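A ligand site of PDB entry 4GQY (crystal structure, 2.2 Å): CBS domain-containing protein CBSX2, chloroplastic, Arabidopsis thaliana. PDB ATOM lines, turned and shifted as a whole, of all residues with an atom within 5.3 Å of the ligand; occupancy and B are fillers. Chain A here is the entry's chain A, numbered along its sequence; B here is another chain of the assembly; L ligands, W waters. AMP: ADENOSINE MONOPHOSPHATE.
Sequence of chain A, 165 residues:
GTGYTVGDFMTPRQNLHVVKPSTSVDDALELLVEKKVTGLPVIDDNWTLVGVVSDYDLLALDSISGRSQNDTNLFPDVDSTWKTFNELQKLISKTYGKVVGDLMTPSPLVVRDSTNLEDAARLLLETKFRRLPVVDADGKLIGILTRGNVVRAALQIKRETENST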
ATOM      1  N   THR A  38      -7.296  -8.954   1.641  1.00  0.00           N
ATOM      2  CA  THR A  38      -7.392  -9.645   0.363  1.00  0.00           C
ATOM      3  C   THR A  38      -8.797  -9.561  -0.201  1.00  0.00           C
ATOM      4  O   THR A  38      -9.040 -10.053  -1.297  1.00  0.00           O
ATOM      5  CB  THR A  38      -7.036 -11.116   0.550  1.00  0.00           C
ATOM      6  OG1 THR A  38      -7.840 -11.664   1.604  1.00  0.00           O
ATOM      7  CG2 THR A  38      -5.576 -11.256   0.925  1.00  0.00           C
ATOM      8  N   VAL A  52     -19.551  -9.736  -1.677  1.00  0.00           N
ATOM      9  CA  VAL A  52     -18.138  -9.759  -1.345  1.00  0.00           C
ATOM     10  C   VAL A  52     -17.364  -9.354  -2.587  1.00  0.00           C
ATOM     11  O   VAL A  52     -17.641  -9.843  -3.690  1.00  0.00           O
ATOM     12  CB  VAL A  52     -17.662 -11.146  -0.840  1.00  0.00           C
ATOM     13  CG1 VAL A  52     -17.934 -12.247  -1.869  1.00  0.00           C
ATOM     14  CG2 VAL A  52     -16.167 -11.097  -0.527  1.00  0.00           C
ATOM     15  N   VAL A  53     -16.422  -8.429  -2.431  1.00  0.00           N
ATOM     16  CA  VAL A  53     -15.509  -8.150  -3.542  1.00  0.00           C
ATOM     17  C   VAL A  53     -14.090  -8.537  -3.122  1.00  0.00           C
ATOM     18  O   VAL A  53     -13.632  -8.168  -2.050  1.00  0.00           O
ATOM     19  CB  VAL A  53     -15.619  -6.685  -4.038  1.00  0.00           C
ATOM     20  CG1 VAL A  53     -15.226  -5.708  -2.958  1.00  0.00           C
ATOM     21  CG2 VAL A  53     -14.798  -6.496  -5.303  1.00  0.00           C
ATOM     22  N   SER A  54     -13.428  -9.309  -3.965  1.00  0.00           N
ATOM     23  CA  SER A  54     -12.134  -9.882  -3.641  1.00  0.00           C
ATOM     24  C   SER A  54     -11.051  -9.309  -4.554  1.00  0.00           C
ATOM     25  O   SER A  54     -11.367  -8.808  -5.659  1.00  0.00           O
ATOM     26  CB  SER A  54     -12.207 -11.420  -3.770  1.00  0.00           C
ATOM     27  OG  SER A  54     -10.940 -12.010  -3.978  1.00  0.00           O
ATOM     28  N   ASP A  55      -9.795  -9.357  -4.111  1.00  0.00           N
ATOM     29  CA  ASP A  55      -8.678  -9.112  -5.026  1.00  0.00           C
ATOM     30  C   ASP A  55      -8.826  -9.955  -6.307  1.00  0.00           C
ATOM     31  O   ASP A  55      -8.498  -9.497  -7.417  1.00  0.00           O
ATOM     32  CB  ASP A  55      -7.306  -9.316  -4.357  1.00  0.00           C
ATOM     33  CG  ASP A  55      -7.149 -10.710  -3.696  1.00  0.00           C
ATOM     34  OD1 ASP A  55      -7.916 -11.673  -4.014  1.00  0.00           O
ATOM     35  OD2 ASP A  55      -6.228 -10.854  -2.841  1.00  0.00           O
ATOM     36  N   TYR A  56      -9.377 -11.164  -6.165  1.00  0.00           N
ATOM     37  CA  TYR A  56      -9.646 -12.007  -7.326  1.00  0.00           C
ATOM     38  C   TYR A  56     -10.500 -11.269  -8.323  1.00  0.00           C
ATOM     39  O   TYR A  56     -10.212 -11.288  -9.534  1.00  0.00           O
ATOM     40  CB  TYR A  56     -10.368 -13.299  -6.950  1.00  0.00           C
ATOM     41  CG  TYR A  56     -10.512 -14.229  -8.146  1.00  0.00           C
ATOM     42  CD1 TYR A  56      -9.417 -14.906  -8.656  1.00  0.00           C
ATOM     43  CD2 TYR A  56     -11.738 -14.399  -8.780  1.00  0.00           C
ATOM     44  CE1 TYR A  56      -9.521 -15.734  -9.756  1.00  0.00           C
ATOM     45  CE2 TYR A  56     -11.864 -15.233  -9.889  1.00  0.00           C
ATOM     46  CZ  TYR A  56     -10.755 -15.897 -10.354  1.00  0.00           C
ATOM     47  OH  TYR A  56     -10.883 -16.724 -11.450  1.00  0.00           O
ATOM     48  N   ASP A  57     -11.554 -10.630  -7.825  1.00  0.00           N
ATOM     49  CA  ASP A  57     -12.474  -9.869  -8.673  1.00  0.00           C
ATOM     50  C   ASP A  57     -11.796  -8.666  -9.344  1.00  0.00           C
ATOM     51  O   ASP A  57     -12.094  -8.358 -10.491  1.00  0.00           O
ATOM     52  CB  ASP A  57     -13.677  -9.418  -7.837  1.00  0.00           C
ATOM     53  CG  ASP A  57     -14.393 -10.589  -7.166  1.00  0.00           C
ATOM     54  OD1 ASP A  57     -14.672 -11.575  -7.883  1.00  0.00           O
ATOM     55  OD2 ASP A  57     -14.639 -10.539  -5.924  1.00  0.00           O
ATOM     56  N   LYS A  94     -17.069  -6.994 -14.926  1.00  0.00           N
ATOM     57  CA  LYS A  94     -15.865  -6.954 -14.130  1.00  0.00           C
ATOM     58  C   LYS A  94     -14.755  -6.251 -14.874  1.00  0.00           C
ATOM     59  O   LYS A  94     -13.950  -5.544 -14.260  1.00  0.00           O
ATOM     60  CB  LYS A  94     -15.407  -8.351 -13.761  1.00  0.00           C
ATOM     61  CG  LYS A  94     -16.170  -8.982 -12.627  1.00  0.00           C
ATOM     62  CD  LYS A  94     -15.514 -10.308 -12.299  1.00  0.00           C
ATOM     63  CE  LYS A  94     -15.876 -10.798 -10.913  1.00  0.00           C
ATOM     64  NZ  LYS A  94     -15.082 -12.015 -10.575  1.00  0.00           N
ATOM     65  N   MET A 104     -18.492  -7.188  -7.581  1.00  0.00           N
ATOM     66  CA  MET A 104     -18.748  -8.064  -6.441  1.00  0.00           C
ATOM     67  C   MET A 104     -19.455  -9.358  -6.805  1.00  0.00           C
ATOM     68  O   MET A 104     -20.095  -9.458  -7.841  1.00  0.00           O
ATOM     69  CB  MET A 104     -19.578  -7.334  -5.363  1.00  0.00           C
ATOM     70  CG  MET A 104     -21.046  -7.244  -5.669  1.00  0.00           C
ATOM     71  SD  MET A 104     -21.863  -6.090  -4.545  1.00  0.00           S
ATOM     72  CE  MET A 104     -23.562  -6.644  -4.766  1.00  0.00           C
ATOM     73  N   THR A 105     -19.310 -10.358  -5.944  1.00  0.00           N
ATOM     74  CA  THR A 105     -20.153 -11.539  -6.050  1.00  0.00           C
ATOM     75  C   THR A 105     -21.337 -11.240  -5.139  1.00  0.00           C
ATOM     76  O   THR A 105     -21.148 -10.959  -3.955  1.00  0.00           O
ATOM     77  CB  THR A 105     -19.412 -12.783  -5.590  1.00  0.00           C
ATOM     78  OG1 THR A 105     -18.225 -12.950  -6.387  1.00  0.00           O
ATOM     79  CG2 THR A 105     -20.310 -14.038  -5.720  1.00  0.00           C
ATOM     80  N   SER A 107     -24.796 -11.936  -2.855  1.00  0.00           N
ATOM     81  CA  SER A 107     -25.244 -13.067  -2.013  1.00  0.00           C
ATOM     82  C   SER A 107     -24.200 -14.132  -1.736  1.00  0.00           C
ATOM     83  O   SER A 107     -24.361 -15.274  -2.151  1.00  0.00           O
ATOM     84  CB  SER A 107     -26.420 -13.787  -2.675  1.00  0.00           C
ATOM     85  OG  SER A 107     -27.443 -12.900  -3.035  1.00  0.00           O
ATOM     86  N   PRO A 108     -23.134 -13.788  -1.007  1.00  0.00           N
ATOM     87  CA  PRO A 108     -22.107 -14.808  -0.768  1.00  0.00           C
ATOM     88  C   PRO A 108     -22.563 -15.878   0.211  1.00  0.00           C
ATOM     89  O   PRO A 108     -23.549 -15.674   0.915  1.00  0.00           O
ATOM     90  CB  PRO A 108     -20.949 -14.015  -0.159  1.00  0.00           C
ATOM     91  CG  PRO A 108     -21.577 -12.787   0.425  1.00  0.00           C
ATOM     92  CD  PRO A 108     -22.772 -12.472  -0.443  1.00  0.00           C
ATOM     93  N   LEU A 109     -21.858 -17.011   0.254  1.00  0.00           N
ATOM     94  CA  LEU A 109     -22.069 -17.981   1.317  1.00  0.00           C
ATOM     95  C   LEU A 109     -21.585 -17.355   2.608  1.00  0.00           C
ATOM     96  O   LEU A 109     -20.557 -16.669   2.636  1.00  0.00           O
ATOM     97  CB  LEU A 109     -21.268 -19.264   1.058  1.00  0.00           C
ATOM     98  CG  LEU A 109     -21.648 -20.119  -0.148  1.00  0.00           C
ATOM     99  CD1 LEU A 109     -20.890 -21.432  -0.140  1.00  0.00           C
ATOM    100  CD2 LEU A 109     -23.146 -20.344  -0.186  1.00  0.00           C
ATOM    101  N   VAL A 110     -22.330 -17.611   3.693  1.00  0.00           N
ATOM    102  CA  VAL A 110     -22.038 -17.014   4.984  1.00  0.00           C
ATOM    103  C   VAL A 110     -22.236 -18.014   6.108  1.00  0.00           C
ATOM    104  O   VAL A 110     -22.853 -19.062   5.914  1.00  0.00           O
ATOM    105  CB  VAL A 110     -22.906 -15.782   5.261  1.00  0.00           C
ATOM    106  CG1 VAL A 110     -22.717 -14.725   4.169  1.00  0.00           C
ATOM    107  CG2 VAL A 110     -24.389 -16.175   5.414  1.00  0.00           C
ATOM    108  N   LYS A 128     -13.117 -23.591  -1.066  1.00  0.00           N
ATOM    109  CA  LYS A 128     -11.832 -22.933  -1.274  1.00  0.00           C
ATOM    110  C   LYS A 128     -11.850 -21.409  -1.169  1.00  0.00           C
ATOM    111  O   LYS A 128     -10.848 -20.777  -1.477  1.00  0.00           O
ATOM    112  CB  LYS A 128     -11.212 -23.358  -2.632  1.00  0.00           C
ATOM    113  CG  LYS A 128     -10.780 -24.830  -2.687  1.00  0.00           C
ATOM    114  CD  LYS A 128     -10.975 -25.425  -4.095  1.00  0.00           C
ATOM    115  CE  LYS A 128     -10.519 -26.878  -4.141  1.00  0.00           C
ATOM    116  NZ  LYS A 128     -10.663 -27.485  -5.492  1.00  0.00           N
ATOM    117  N   PHE A 129     -12.948 -20.816  -0.702  1.00  0.00           N
ATOM    118  CA  PHE A 129     -12.996 -19.348  -0.537  1.00  0.00           C
ATOM    119  C   PHE A 129     -11.943 -18.888   0.453  1.00  0.00           C
ATOM    120  O   PHE A 129     -11.594 -19.628   1.372  1.00  0.00           O
ATOM    121  CB  PHE A 129     -14.385 -18.860  -0.084  1.00  0.00           C
ATOM    122  CG  PHE A 129     -15.475 -19.054  -1.102  1.00  0.00           C
ATOM    123  CD1 PHE A 129     -15.239 -18.868  -2.459  1.00  0.00           C
ATOM    124  CD2 PHE A 129     -16.761 -19.425  -0.705  1.00  0.00           C
ATOM    125  CE1 PHE A 129     -16.261 -19.040  -3.403  1.00  0.00           C
ATOM    126  CE2 PHE A 129     -17.783 -19.597  -1.650  1.00  0.00           C
ATOM    127  CZ  PHE A 129     -17.526 -19.420  -2.997  1.00  0.00           C
ATOM    128  N   ARG A 130     -11.437 -17.661   0.275  1.00  0.00           N
ATOM    129  CA  ARG A 130     -10.520 -17.098   1.273  1.00  0.00           C
ATOM    130  C   ARG A 130     -11.237 -16.743   2.588  1.00  0.00           C
ATOM    131  O   ARG A 130     -10.652 -16.845   3.665  1.00  0.00           O
ATOM    132  CB  ARG A 130      -9.804 -15.851   0.716  1.00  0.00           C
ATOM    133  CG  ARG A 130      -9.025 -15.024   1.768  1.00  0.00           C
ATOM    134  CD  ARG A 130      -7.879 -15.827   2.406  1.00  0.00           C
ATOM    135  NE  ARG A 130      -6.946 -16.317   1.381  1.00  0.00           N
ATOM    136  CZ  ARG A 130      -5.905 -17.125   1.607  1.00  0.00           C
ATOM    137  NH1 ARG A 130      -5.624 -17.540   2.847  1.00  0.00           N
ATOM    138  NH2 ARG A 130      -5.138 -17.518   0.588  1.00  0.00           N
ATOM    139  N   ARG A 131     -12.492 -16.326   2.493  1.00  0.00           N
ATOM    140  CA  ARG A 131     -13.203 -15.820   3.672  1.00  0.00           C
ATOM    141  C   ARG A 131     -14.689 -16.189   3.686  1.00  0.00           C
ATOM    142  O   ARG A 131     -15.313 -16.340   2.641  1.00  0.00           O
ATOM    143  CB  ARG A 131     -13.068 -14.307   3.752  1.00  0.00           C
ATOM    144  CG  ARG A 131     -13.756 -13.592   2.583  1.00  0.00           C
ATOM    145  CD  ARG A 131     -13.288 -12.164   2.440  1.00  0.00           C
ATOM    146  NE  ARG A 131     -11.871 -12.067   2.100  1.00  0.00           N
ATOM    147  CZ  ARG A 131     -11.360 -12.380   0.899  1.00  0.00           C
ATOM    148  NH1 ARG A 131     -12.128 -12.841  -0.091  1.00  0.00           N
ATOM    149  NH2 ARG A 131     -10.055 -12.249   0.701  1.00  0.00           N
ATOM    150  N   LEU A 132     -15.237 -16.320   4.890  1.00  0.00           N
ATOM    151  CA  LEU A 132     -16.668 -16.413   5.110  1.00  0.00           C
ATOM    152  C   LEU A 132     -17.117 -15.188   5.876  1.00  0.00           C
ATOM    153  O   LEU A 132     -16.722 -14.994   7.038  1.00  0.00           O
ATOM    154  CB  LEU A 132     -17.006 -17.652   5.918  1.00  0.00           C
ATOM    155  CG  LEU A 132     -16.624 -18.878   5.108  1.00  0.00           C
ATOM    156  CD1 LEU A 132     -16.681 -20.132   5.957  1.00  0.00           C
ATOM    157  CD2 LEU A 132     -17.584 -18.916   3.956  1.00  0.00           C
ATOM    158  N   PRO A 133     -17.916 -14.355   5.231  1.00  0.00           N
ATOM    159  CA  PRO A 133     -18.505 -13.225   5.953  1.00  0.00           C
ATOM    160  C   PRO A 133     -19.449 -13.826   7.006  1.00  0.00           C
ATOM    161  O   PRO A 133     -20.051 -14.868   6.770  1.00  0.00           O
ATOM    162  CB  PRO A 133     -19.307 -12.497   4.880  1.00  0.00           C
ATOM    163  CG  PRO A 133     -18.751 -12.974   3.576  1.00  0.00           C
ATOM    164  CD  PRO A 133     -18.395 -14.426   3.850  1.00  0.00           C
ATOM    165  N   ARG B 130      -2.988 -18.368  -5.241  1.00  0.00           N
ATOM    166  CA  ARG B 130      -2.768 -17.166  -4.453  1.00  0.00           C
ATOM    167  C   ARG B 130      -1.476 -16.463  -4.836  1.00  0.00           C
ATOM    168  O   ARG B 130      -1.391 -15.244  -4.775  1.00  0.00           O
ATOM    169  CB  ARG B 130      -2.761 -17.494  -2.956  1.00  0.00           C
ATOM    170  CG  ARG B 130      -4.030 -18.229  -2.502  1.00  0.00           C
ATOM    171  CD  ARG B 130      -5.285 -17.419  -2.726  1.00  0.00           C
ATOM    172  NE  ARG B 130      -6.543 -18.161  -2.645  1.00  0.00           N
ATOM    173  CZ  ARG B 130      -7.677 -17.607  -2.245  1.00  0.00           C
ATOM    174  NH1 ARG B 130      -7.662 -16.318  -1.866  1.00  0.00           N
ATOM    175  NH2 ARG B 130      -8.807 -18.309  -2.191  1.00  0.00           N
ATOM    176  N   ARG B 147      -1.516 -12.003  -5.683  1.00  0.00           N
ATOM    177  CA  ARG B 147      -2.618 -11.137  -6.069  1.00  0.00           C
ATOM    178  C   ARG B 147      -2.426  -9.730  -5.504  1.00  0.00           C
ATOM    179  O   ARG B 147      -2.687  -8.746  -6.194  1.00  0.00           O
ATOM    180  CB  ARG B 147      -3.915 -11.694  -5.525  1.00  0.00           C
ATOM    181  CG  ARG B 147      -4.365 -13.017  -6.125  1.00  0.00           C
ATOM    182  CD  ARG B 147      -5.830 -13.289  -5.709  1.00  0.00           C
ATOM    183  NE  ARG B 147      -6.255 -14.655  -5.982  1.00  0.00           N
ATOM    184  CZ  ARG B 147      -7.286 -15.262  -5.396  1.00  0.00           C
ATOM    185  NH1 ARG B 147      -8.018 -14.614  -4.501  1.00  0.00           N
ATOM    186  NH2 ARG B 147      -7.593 -16.508  -5.726  1.00  0.00           N
HETATM  187  P   AMP L   1     -11.401 -15.498  -3.029  1.00  0.00           P
HETATM  188  O1P AMP L   1     -10.299 -16.198  -3.796  1.00  0.00           O
HETATM  189  O2P AMP L   1     -12.098 -16.366  -1.985  1.00  0.00           O
HETATM  190  O3P AMP L   1     -10.982 -14.121  -2.539  1.00  0.00           O
HETATM  191  O5' AMP L   1     -12.526 -15.163  -4.103  1.00  0.00           O
HETATM  192  C5' AMP L   1     -12.733 -15.983  -5.242  1.00  0.00           C
HETATM  193  C4' AMP L   1     -14.055 -15.684  -5.892  1.00  0.00           C
HETATM  194  O4' AMP L   1     -15.134 -16.186  -5.052  1.00  0.00           O
HETATM  195  C3' AMP L   1     -14.358 -14.202  -6.125  1.00  0.00           C
HETATM  196  O3' AMP L   1     -15.197 -14.065  -7.275  1.00  0.00           O
HETATM  197  C2' AMP L   1     -15.186 -13.830  -4.889  1.00  0.00           C
HETATM  198  O2' AMP L   1     -16.032 -12.718  -5.084  1.00  0.00           O
HETATM  199  C1' AMP L   1     -15.976 -15.122  -4.632  1.00  0.00           C
HETATM  200  N9  AMP L   1     -16.269 -15.341  -3.218  1.00  0.00           N
HETATM  201  C8  AMP L   1     -15.378 -15.117  -2.226  1.00  0.00           C
HETATM  202  N7  AMP L   1     -15.900 -15.413  -1.013  1.00  0.00           N
HETATM  203  C5  AMP L   1     -17.157 -15.831  -1.220  1.00  0.00           C
HETATM  204  C6  AMP L   1     -18.275 -16.266  -0.368  1.00  0.00           C
HETATM  205  N6  AMP L   1     -18.108 -16.341   0.977  1.00  0.00           N
HETATM  206  N1  AMP L   1     -19.433 -16.619  -0.975  1.00  0.00           N
HETATM  207  C2  AMP L   1     -19.603 -16.551  -2.308  1.00  0.00           C
HETATM  208  N3  AMP L   1     -18.628 -16.141  -3.137  1.00  0.00           N
HETATM  209  C4  AMP L   1     -17.415 -15.768  -2.664  1.00  0.00           C
HETATM  210  O   HOH W   1      -8.898 -13.133  -1.405  1.00  0.00           O
HETATM  211  O   HOH W   2     -18.721 -17.285  -5.837  1.00  0.00           O
HETATM  212  O   HOH W   3     -17.020 -15.951  -8.497  1.00  0.00           O
HETATM  213  O   HOH W   4     -13.257 -15.475   0.133  1.00  0.00           O
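Water W1 lies within hydrogen-bond range of NH2 of Arg 131, O3P of the ligand, O of Thr 38, OD1 of Asp 55, NH1 of Arg 130 of chain B and OG of Ser 54.
Water W4 lies within hydrogen-bond range of an oxygen (O2P) of the ligand, the backbone NH (N) of Arg 131 and the backbone NH (N) of Arg 130 of chain A.
The side-chain hydroxyl (OG) of Ser 54 sits at hydrogen-bond distance from the backbone NH (N) of Tyr 56 (2.8 Å).
The guanidinium group (NH2) of Arg 130 of chain B is in hydrogen-bond range of the backbone carbonyl oxygen (O) of Lys 128 (3.3 Å).
The side-chain carboxylate (OD1) of Asp 55 lies within salt-bridge range of the guanidinium group (NH1) of Arg 147 of chain B, at 3.0 Å.
The side-chain carboxylate (OD1) of Asp 55 lies within hydrogen-bond range of the side-chain hydroxyl (OG) of Ser 54 (3.0 Å).
N of Thr 105 sits at hydrogen-bond distance from O of Val 52 (2.9 Å).
The guanidinium group (NH2) of Arg 131 lies within hydrogen-bond range of the side-chain hydroxyl (OG1) of Thr 38 (2.5 Å).
The side-chain carboxylate (OD1) of Asp 57 lies within salt-bridge range of the side-chain amino group (NZ) of Lys 94, 2.8 Å away.
The backbone NH of Arg 147 of chain B sits at hydrogen-bond distance from the backbone carbonyl oxygen of Arg 130 of chain B (3.4 Å).
O of Val 52 touches O2' of the ligand (3.6 Å).
Tyr 56 touches the ligand.
NZ of Lys 94 touches O3' of the ligand (3.9 Å).
Pro 108 touches the ligand.
CA of Phe 129 touches O2P of the ligand, 3.4 Å away.
Leu 132 touches the ligand.
CD of Pro 133 touches N6 of the ligand (3.5 Å).
Hydrophobic or aromatic side chains within 4 Å of the ligand: Val 52, Tyr 56, Pro 108, Leu 109, Phe 129, Leu 132 and Pro 133.
The nearest printed residue that does not touch the ligand is Asp 55 (4.2 Å).
O1P of the ligand lies within salt-bridge range of NH2 of Arg 130 of chain B, 3.0 Å away.
A nitrogen (N6) of the ligand is in hydrogen-bond range of the backbone carbonyl oxygen of Arg 131.
O2P of the ligand is in hydrogen-bond range of N of Arg 130 of chain A, 2.7 Å away.
OD1 of Asp 57 lies within hydrogen-bond range of O3' of the ligand (2.6 Å).
An oxygen (O2') of the ligand sits at hydrogen-bond distance from the side-chain hydroxyl (OG1) of Thr 105, at 2.6 Å.
O of Leu 109 lies within hydrogen-bond range of N6 of the ligand.
O3P of the ligand is in salt-bridge range of NH1 of Arg 131, at 3.0 Å.
An oxygen (O1P) of the ligand lies within salt-bridge range of the guanidinium group of Arg 147 of chain B, at 2.9 Å.
The backbone NH (N) of Leu 109 lies within hydrogen-bond range of a nitrogen (N1) of the ligand (2.7 Å).
The side-chain hydroxyl (OG) of Ser 54 lies within hydrogen-bond range of an oxygen (O3P) of the ligand (2.6 Å).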
